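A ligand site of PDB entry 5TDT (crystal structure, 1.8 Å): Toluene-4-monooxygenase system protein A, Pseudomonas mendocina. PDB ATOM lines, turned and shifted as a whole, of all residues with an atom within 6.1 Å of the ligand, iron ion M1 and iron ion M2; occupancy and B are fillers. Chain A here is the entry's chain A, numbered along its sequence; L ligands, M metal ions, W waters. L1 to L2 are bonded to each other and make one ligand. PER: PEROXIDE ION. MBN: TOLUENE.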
ATOM      1  N   ALA A  99      10.299 -38.415  24.974  1.00  0.00           N
ATOM      2  CA  ALA A  99      10.799 -37.222  24.305  1.00  0.00           C
ATOM      3  C   ALA A  99       9.819 -36.047  24.336  1.00  0.00           C
ATOM      4  O   ALA A  99      10.256 -34.897  24.188  1.00  0.00           O
ATOM      5  CB  ALA A  99      11.168 -37.558  22.852  1.00  0.00           C
ATOM      6  N   ILE A 100       8.526 -36.288  24.554  1.00  0.00           N
ATOM      7  CA  ILE A 100       7.487 -35.296  24.295  1.00  0.00           C
ATOM      8  C   ILE A 100       6.795 -34.814  25.570  1.00  0.00           C
ATOM      9  O   ILE A 100       6.532 -33.619  25.694  1.00  0.00           O
ATOM     10  CB  ILE A 100       6.468 -35.850  23.271  1.00  0.00           C
ATOM     11  CG1 ILE A 100       7.112 -36.048  21.890  1.00  0.00           C
ATOM     12  CG2 ILE A 100       5.233 -34.936  23.169  1.00  0.00           C
ATOM     13  CD1 ILE A 100       7.747 -34.801  21.306  1.00  0.00           C
ATOM     14  N   ALA A 101       6.473 -35.714  26.492  1.00  0.00           N
ATOM     15  CA  ALA A 101       5.467 -35.394  27.522  1.00  0.00           C
ATOM     16  C   ALA A 101       5.867 -34.185  28.374  1.00  0.00           C
ATOM     17  O   ALA A 101       5.084 -33.247  28.552  1.00  0.00           O
ATOM     18  CB  ALA A 101       5.194 -36.607  28.406  1.00  0.00           C
ATOM     19  N   VAL A 102       7.079 -34.195  28.927  1.00  0.00           N
ATOM     20  CA  VAL A 102       7.454 -33.084  29.790  1.00  0.00           C
ATOM     21  C   VAL A 102       7.898 -31.876  28.974  1.00  0.00           C
ATOM     22  O   VAL A 102       7.855 -30.751  29.473  1.00  0.00           O
ATOM     23  CB  VAL A 102       8.510 -33.594  30.806  1.00  0.00           C
ATOM     24  CG1 VAL A 102       9.081 -32.443  31.705  1.00  0.00           C
ATOM     25  CG2 VAL A 102       7.873 -34.681  31.674  1.00  0.00           C
ATOM     26  N   GLY A 103       8.257 -32.066  27.700  1.00  0.00           N
ATOM     27  CA  GLY A 103       8.487 -30.931  26.814  1.00  0.00           C
ATOM     28  C   GLY A 103       7.210 -30.193  26.474  1.00  0.00           C
ATOM     29  O   GLY A 103       7.210 -28.974  26.307  1.00  0.00           O
ATOM     30  N   GLU A 104       6.095 -30.922  26.357  1.00  0.00           N
ATOM     31  CA  GLU A 104       4.793 -30.267  26.244  1.00  0.00           C
ATOM     32  C   GLU A 104       4.516 -29.393  27.454  1.00  0.00           C
ATOM     33  O   GLU A 104       4.023 -28.268  27.333  1.00  0.00           O
ATOM     34  CB  GLU A 104       3.688 -31.314  26.101  1.00  0.00           C
ATOM     35  CG  GLU A 104       3.820 -32.148  24.862  1.00  0.00           C
ATOM     36  CD  GLU A 104       2.882 -31.714  23.763  1.00  0.00           C
ATOM     37  OE1 GLU A 104       2.488 -32.581  22.959  1.00  0.00           O
ATOM     38  OE2 GLU A 104       2.517 -30.507  23.716  1.00  0.00           O
ATOM     39  N   ALA A 107       6.210 -26.233  27.187  1.00  0.00           N
ATOM     40  CA  ALA A 107       5.586 -25.297  26.258  1.00  0.00           C
ATOM     41  C   ALA A 107       4.580 -24.381  26.946  1.00  0.00           C
ATOM     42  O   ALA A 107       4.302 -23.288  26.433  1.00  0.00           O
ATOM     43  CB  ALA A 107       4.914 -26.055  25.105  1.00  0.00           C
ATOM     44  N   GLU A 111       4.141 -20.279  26.100  1.00  0.00           N
ATOM     45  CA  GLU A 111       2.878 -19.576  25.968  1.00  0.00           C
ATOM     46  C   GLU A 111       2.704 -18.531  27.077  1.00  0.00           C
ATOM     47  O   GLU A 111       2.218 -17.429  26.837  1.00  0.00           O
ATOM     48  CB  GLU A 111       1.713 -20.585  25.999  1.00  0.00           C
ATOM     49  CG  GLU A 111       1.665 -21.565  24.793  1.00  0.00           C
ATOM     50  CD  GLU A 111       1.198 -20.924  23.481  1.00  0.00           C
ATOM     51  OE1 GLU A 111       0.725 -19.766  23.494  1.00  0.00           O
ATOM     52  OE2 GLU A 111       1.283 -21.606  22.414  1.00  0.00           O
ATOM     53  N   ASP A 133      -3.824 -25.321  26.535  1.00  0.00           N
ATOM     54  CA  ASP A 133      -3.614 -26.434  25.601  1.00  0.00           C
ATOM     55  C   ASP A 133      -2.399 -27.258  26.001  1.00  0.00           C
ATOM     56  O   ASP A 133      -2.445 -28.501  25.988  1.00  0.00           O
ATOM     57  CB  ASP A 133      -3.436 -25.917  24.172  1.00  0.00           C
ATOM     58  CG  ASP A 133      -4.685 -25.291  23.587  1.00  0.00           C
ATOM     59  OD1 ASP A 133      -5.823 -25.498  24.102  1.00  0.00           O
ATOM     60  OD2 ASP A 133      -4.526 -24.588  22.572  1.00  0.00           O
ATOM     61  N   GLU A 134      -1.279 -26.601  26.312  1.00  0.00           N
ATOM     62  CA  GLU A 134      -0.078 -27.395  26.564  1.00  0.00           C
ATOM     63  C   GLU A 134      -0.156 -28.085  27.927  1.00  0.00           C
ATOM     64  O   GLU A 134       0.438 -29.153  28.109  1.00  0.00           O
ATOM     65  CB  GLU A 134       1.181 -26.532  26.456  1.00  0.00           C
ATOM     66  CG  GLU A 134       1.313 -25.773  25.128  1.00  0.00           C
ATOM     67  CD  GLU A 134       1.539 -26.669  23.901  1.00  0.00           C
ATOM     68  OE1 GLU A 134       1.323 -27.912  23.949  1.00  0.00           O
ATOM     69  OE2 GLU A 134       1.954 -26.114  22.857  1.00  0.00           O
ATOM     70  N   HIS A 137      -1.795 -31.212  26.988  1.00  0.00           N
ATOM     71  CA  HIS A 137      -0.936 -32.139  26.267  1.00  0.00           C
ATOM     72  C   HIS A 137       0.075 -32.812  27.192  1.00  0.00           C
ATOM     73  O   HIS A 137       0.341 -34.009  27.051  1.00  0.00           O
ATOM     74  CB  HIS A 137      -0.231 -31.420  25.117  1.00  0.00           C
ATOM     75  CG  HIS A 137      -1.181 -30.789  24.149  1.00  0.00           C
ATOM     76  ND1 HIS A 137      -0.787 -29.903  23.169  1.00  0.00           N
ATOM     77  CD2 HIS A 137      -2.525 -30.928  24.014  1.00  0.00           C
ATOM     78  CE1 HIS A 137      -1.845 -29.513  22.476  1.00  0.00           C
ATOM     79  NE2 HIS A 137      -2.921 -30.123  22.968  1.00  0.00           N
ATOM     80  N   GLN A 141      -0.130 -36.879  28.079  1.00  0.00           N
ATOM     81  CA  GLN A 141       0.991 -37.719  27.682  1.00  0.00           C
ATOM     82  C   GLN A 141       1.814 -38.207  28.864  1.00  0.00           C
ATOM     83  O   GLN A 141       2.766 -38.970  28.660  1.00  0.00           O
ATOM     84  CB  GLN A 141       1.830 -36.976  26.650  1.00  0.00           C
ATOM     85  CG  GLN A 141       1.064 -37.007  25.336  1.00  0.00           C
ATOM     86  CD  GLN A 141       1.651 -36.156  24.262  1.00  0.00           C
ATOM     87  OE1 GLN A 141       2.022 -36.667  23.193  1.00  0.00           O
ATOM     88  NE2 GLN A 141       1.703 -34.854  24.492  1.00  0.00           N
ATOM     89  N   TYR A 162      13.230 -35.926  30.930  1.00  0.00           N
ATOM     90  CA  TYR A 162      13.651 -34.528  30.981  1.00  0.00           C
ATOM     91  C   TYR A 162      14.354 -34.184  32.290  1.00  0.00           C
ATOM     92  O   TYR A 162      14.976 -33.127  32.396  1.00  0.00           O
ATOM     93  CB  TYR A 162      12.444 -33.592  30.774  1.00  0.00           C
ATOM     94  CG  TYR A 162      12.085 -33.345  29.302  1.00  0.00           C
ATOM     95  CD1 TYR A 162      11.602 -34.381  28.513  1.00  0.00           C
ATOM     96  CD2 TYR A 162      12.213 -32.081  28.736  1.00  0.00           C
ATOM     97  CE1 TYR A 162      11.270 -34.167  27.163  1.00  0.00           C
ATOM     98  CE2 TYR A 162      11.866 -31.844  27.397  1.00  0.00           C
ATOM     99  CZ  TYR A 162      11.397 -32.892  26.624  1.00  0.00           C
ATOM    100  OH  TYR A 162      11.069 -32.675  25.297  1.00  0.00           O
ATOM    101  N   PHE A 176      14.414 -27.347  23.047  1.00  0.00           N
ATOM    102  CA  PHE A 176      13.216 -26.728  23.598  1.00  0.00           C
ATOM    103  C   PHE A 176      13.535 -25.558  24.526  1.00  0.00           C
ATOM    104  O   PHE A 176      12.778 -24.577  24.554  1.00  0.00           O
ATOM    105  CB  PHE A 176      12.348 -27.756  24.322  1.00  0.00           C
ATOM    106  CG  PHE A 176      11.673 -28.731  23.405  1.00  0.00           C
ATOM    107  CD1 PHE A 176      10.998 -28.289  22.264  1.00  0.00           C
ATOM    108  CD2 PHE A 176      11.749 -30.086  23.627  1.00  0.00           C
ATOM    109  CE1 PHE A 176      10.386 -29.185  21.400  1.00  0.00           C
ATOM    110  CE2 PHE A 176      11.145 -30.981  22.770  1.00  0.00           C
ATOM    111  CZ  PHE A 176      10.475 -30.535  21.653  1.00  0.00           C
ATOM    112  N   ILE A 180      11.655 -22.458  23.141  1.00  0.00           N
ATOM    113  CA  ILE A 180      10.423 -22.335  23.926  1.00  0.00           C
ATOM    114  C   ILE A 180      10.629 -21.458  25.171  1.00  0.00           C
ATOM    115  O   ILE A 180       9.925 -20.461  25.359  1.00  0.00           O
ATOM    116  CB  ILE A 180       9.850 -23.716  24.320  1.00  0.00           C
ATOM    117  CG1 ILE A 180       9.482 -24.515  23.074  1.00  0.00           C
ATOM    118  CG2 ILE A 180       8.647 -23.523  25.254  1.00  0.00           C
ATOM    119  CD1 ILE A 180       8.822 -25.837  23.376  1.00  0.00           C
ATOM    120  N   LEU A 192       8.576 -21.047  18.035  1.00  0.00           N
ATOM    121  CA  LEU A 192       7.722 -22.136  18.522  1.00  0.00           C
ATOM    122  C   LEU A 192       6.449 -22.222  17.683  1.00  0.00           C
ATOM    123  O   LEU A 192       6.253 -23.194  16.948  1.00  0.00           O
ATOM    124  CB  LEU A 192       7.389 -21.933  19.998  1.00  0.00           C
ATOM    125  CG  LEU A 192       6.302 -22.867  20.574  1.00  0.00           C
ATOM    126  CD1 LEU A 192       6.702 -24.345  20.463  1.00  0.00           C
ATOM    127  CD2 LEU A 192       5.991 -22.518  22.023  1.00  0.00           C
ATOM    128  N   PHE A 196       8.037 -24.435  14.570  1.00  0.00           N
ATOM    129  CA  PHE A 196       7.928 -25.792  15.087  1.00  0.00           C
ATOM    130  C   PHE A 196       6.484 -26.309  15.006  1.00  0.00           C
ATOM    131  O   PHE A 196       6.245 -27.440  14.570  1.00  0.00           O
ATOM    132  CB  PHE A 196       8.433 -25.823  16.522  1.00  0.00           C
ATOM    133  CG  PHE A 196       8.438 -27.178  17.152  1.00  0.00           C
ATOM    134  CD1 PHE A 196       9.222 -28.195  16.608  1.00  0.00           C
ATOM    135  CD2 PHE A 196       7.696 -27.435  18.291  1.00  0.00           C
ATOM    136  CE1 PHE A 196       9.227 -29.463  17.196  1.00  0.00           C
ATOM    137  CE2 PHE A 196       7.707 -28.683  18.871  1.00  0.00           C
ATOM    138  CZ  PHE A 196       8.473 -29.700  18.330  1.00  0.00           C
ATOM    139  N   GLU A 197       5.502 -25.478  15.391  1.00  0.00           N
ATOM    140  CA  GLU A 197       4.143 -25.969  15.610  1.00  0.00           C
ATOM    141  C   GLU A 197       3.275 -26.000  14.344  1.00  0.00           C
ATOM    142  O   GLU A 197       2.299 -26.767  14.318  1.00  0.00           O
ATOM    143  CB  GLU A 197       3.442 -25.156  16.690  1.00  0.00           C
ATOM    144  CG  GLU A 197       4.057 -25.393  18.083  1.00  0.00           C
ATOM    145  CD  GLU A 197       3.287 -24.750  19.229  1.00  0.00           C
ATOM    146  OE1 GLU A 197       2.835 -23.596  19.105  1.00  0.00           O
ATOM    147  OE2 GLU A 197       3.122 -25.406  20.273  1.00  0.00           O
ATOM    148  N   THR A 201       5.716 -30.497  14.033  1.00  0.00           N
ATOM    149  CA  THR A 201       4.965 -31.406  14.895  1.00  0.00           C
ATOM    150  C   THR A 201       3.976 -32.263  14.113  1.00  0.00           C
ATOM    151  O   THR A 201       3.603 -33.350  14.563  1.00  0.00           O
ATOM    152  CB  THR A 201       4.226 -30.661  16.009  1.00  0.00           C
ATOM    153  OG1 THR A 201       3.369 -29.669  15.430  1.00  0.00           O
ATOM    154  CG2 THR A 201       5.224 -29.994  16.966  1.00  0.00           C
ATOM    155  N   PHE A 205       2.885 -36.076  15.190  1.00  0.00           N
ATOM    156  CA  PHE A 205       1.541 -36.231  15.724  1.00  0.00           C
ATOM    157  C   PHE A 205       0.499 -36.637  14.689  1.00  0.00           C
ATOM    158  O   PHE A 205      -0.619 -37.012  15.077  1.00  0.00           O
ATOM    159  CB  PHE A 205       1.084 -34.937  16.412  1.00  0.00           C
ATOM    160  CG  PHE A 205       1.746 -34.705  17.736  1.00  0.00           C
ATOM    161  CD1 PHE A 205       3.049 -34.212  17.792  1.00  0.00           C
ATOM    162  CD2 PHE A 205       1.081 -34.985  18.914  1.00  0.00           C
ATOM    163  CE1 PHE A 205       3.670 -33.985  19.027  1.00  0.00           C
ATOM    164  CE2 PHE A 205       1.695 -34.773  20.144  1.00  0.00           C
ATOM    165  CZ  PHE A 205       3.003 -34.274  20.194  1.00  0.00           C
ATOM    166  N   ILE A 227      -4.665 -34.179  20.094  1.00  0.00           N
ATOM    167  CA  ILE A 227      -3.728 -33.168  20.545  1.00  0.00           C
ATOM    168  C   ILE A 227      -3.436 -32.189  19.413  1.00  0.00           C
ATOM    169  O   ILE A 227      -3.417 -30.964  19.601  1.00  0.00           O
ATOM    170  CB  ILE A 227      -2.451 -33.860  21.067  1.00  0.00           C
ATOM    171  CG1 ILE A 227      -2.735 -34.470  22.445  1.00  0.00           C
ATOM    172  CG2 ILE A 227      -1.262 -32.896  21.075  1.00  0.00           C
ATOM    173  CD1 ILE A 227      -1.599 -35.355  22.965  1.00  0.00           C
ATOM    174  N   ASP A 230      -5.573 -29.053  18.855  1.00  0.00           N
ATOM    175  CA  ASP A 230      -5.223 -27.862  19.632  1.00  0.00           C
ATOM    176  C   ASP A 230      -4.060 -27.115  18.987  1.00  0.00           C
ATOM    177  O   ASP A 230      -4.075 -25.880  18.892  1.00  0.00           O
ATOM    178  CB  ASP A 230      -4.846 -28.233  21.087  1.00  0.00           C
ATOM    179  CG  ASP A 230      -5.960 -28.964  21.838  1.00  0.00           C
ATOM    180  OD1 ASP A 230      -5.623 -29.871  22.611  1.00  0.00           O
ATOM    181  OD2 ASP A 230      -7.158 -28.624  21.660  1.00  0.00           O
ATOM    182  N   GLU A 231      -3.010 -27.856  18.636  1.00  0.00           N
ATOM    183  CA  GLU A 231      -1.842 -27.269  17.979  1.00  0.00           C
ATOM    184  C   GLU A 231      -2.267 -26.411  16.797  1.00  0.00           C
ATOM    185  O   GLU A 231      -1.787 -25.277  16.634  1.00  0.00           O
ATOM    186  CB  GLU A 231      -0.897 -28.388  17.528  1.00  0.00           C
ATOM    187  CG  GLU A 231       0.366 -27.888  16.857  1.00  0.00           C
ATOM    188  CD  GLU A 231       1.498 -27.682  17.839  1.00  0.00           C
ATOM    189  OE1 GLU A 231       2.567 -28.312  17.670  1.00  0.00           O
ATOM    190  OE2 GLU A 231       1.306 -26.902  18.787  1.00  0.00           O
ATOM    191  N   HIS A 234      -3.540 -22.918  18.262  1.00  0.00           N
ATOM    192  CA  HIS A 234      -2.647 -21.940  18.894  1.00  0.00           C
ATOM    193  C   HIS A 234      -1.354 -21.721  18.101  1.00  0.00           C
ATOM    194  O   HIS A 234      -0.695 -20.699  18.319  1.00  0.00           O
ATOM    195  CB  HIS A 234      -2.343 -22.301  20.367  1.00  0.00           C
ATOM    196  CG  HIS A 234      -1.538 -23.544  20.571  1.00  0.00           C
ATOM    197  ND1 HIS A 234      -1.994 -24.602  21.334  1.00  0.00           N
ATOM    198  CD2 HIS A 234      -0.278 -23.875  20.190  1.00  0.00           C
ATOM    199  CE1 HIS A 234      -1.071 -25.553  21.375  1.00  0.00           C
ATOM    200  NE2 HIS A 234      -0.019 -25.127  20.687  1.00  0.00           N
ATOM    201  N   ALA A 235      -1.016 -22.606  17.162  1.00  0.00           N
ATOM    202  CA  ALA A 235       0.093 -22.317  16.259  1.00  0.00           C
ATOM    203  C   ALA A 235      -0.196 -21.114  15.352  1.00  0.00           C
ATOM    204  O   ALA A 235       0.737 -20.498  14.849  1.00  0.00           O
ATOM    205  CB  ALA A 235       0.436 -23.536  15.390  1.00  0.00           C
HETATM  206  O1  PER L   1       3.374 -28.831  21.161  1.00  0.00           O
HETATM  207  O2  PER L   1       3.541 -27.921  22.225  1.00  0.00           O
HETATM  208  C   MBN L   2       7.565 -31.529  22.986  1.00  0.00           C
HETATM  209  C1  MBN L   2       6.572 -30.601  22.312  1.00  0.00           C
HETATM  210  C2  MBN L   2       6.547 -29.271  22.691  1.00  0.00           C
HETATM  211  C3  MBN L   2       5.657 -28.413  22.079  1.00  0.00           C
HETATM  212  C4  MBN L   2       4.753 -28.879  21.127  1.00  0.00           C
HETATM  213  C5  MBN L   2       4.785 -30.222  20.756  1.00  0.00           C
HETATM  214  C6  MBN L   2       5.695 -31.083  21.349  1.00  0.00           C
HETATM  215 FE    FE M   1       1.293 -29.375  22.499  1.00  0.00          FE
HETATM  216 FE    FE M   2       1.692 -26.617  20.809  1.00  0.00          FE
HETATM  217  O   HOH W   1       0.585 -28.169  20.882  1.00  0.00           O
HETATM  218  O   HOH W   2       1.301 -30.962  21.232  1.00  0.00           O
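The backbone carbonyl oxygen of Glu 197 sits at hydrogen-bond distance from the side-chain hydroxyl of Thr 201 (3.3 Å). N of Glu 197 is in hydrogen-bond range of O of Leu 192 (2.9 Å). The side-chain amide nitrogen (NE2) of Gln 141 lies within hydrogen-bond range of the side-chain carboxylate (OE1) of Glu 104, 2.9 Å away. The side-chain hydroxyl (OG1) of Thr 201 is in hydrogen-bond range of the side-chain carboxylate (OE1) of Glu 231 (2.7 Å). O of Asp 133 lies close to NE2 of His 137 (3.5 Å). A ring nitrogen (NE2) of His 137 is in hydrogen-bond range of the side-chain carboxylate (OD1) of Asp 230 (2.7 Å). ND1 of His 234 is in hydrogen-bond range of OD2 of Asp 133, 2.8 Å away. O of Phe 196 sits at hydrogen-bond distance from N of Thr 201, at 3.1 Å.
Residues that only touch the ligand: Phe 176, Ile 100, Gly 103, Ala 107, Phe 196 and Thr 201. Hydrophobic or aromatic side chains within 4 Å of the ligand: Ile 100, Ala 107, Phe 176 and Phe 196. Within 4 Å of the ligand: Ile 100, Gly 103, Glu 104, Ala 107, Glu 134, Phe 176, Phe 196, Glu 197, Thr 201 and Glu 231.
Within 4 Å of iron ion M1: Glu 104, Glu 134 and His 137.
Within 4 Å of iron ion M2: Glu 134, Glu 197, Glu 231 and His 234. Along chain A the residues within 4 Å of iron ion M2 span positions 134 to 234. The nearest printed residue that does not touch iron ion M2 is His 137 (4.7 Å).
Iron ion M1 is bound by water W2 (2.0 Å), OE1 of Glu 134 (2.1 Å), OE2 of Glu 104 (2.1 Å), water W1 (2.1 Å), ND1 of His 137 (2.2 Å) and O1 of PER L1 (2.5 Å).
Iron ion M2 is bound by water W1 (1.9 Å), OE2 of Glu 197 (1.9 Å), OE2 of Glu 231 (2.1 Å), OE2 of Glu 134 (2.1 Å) and NE2 of His 234 (2.3 Å). Iron ion M2 has five donor atoms within binding distance. Slightly farther from iron ion M2 lies O2 of PER L1 (2.7 Å).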
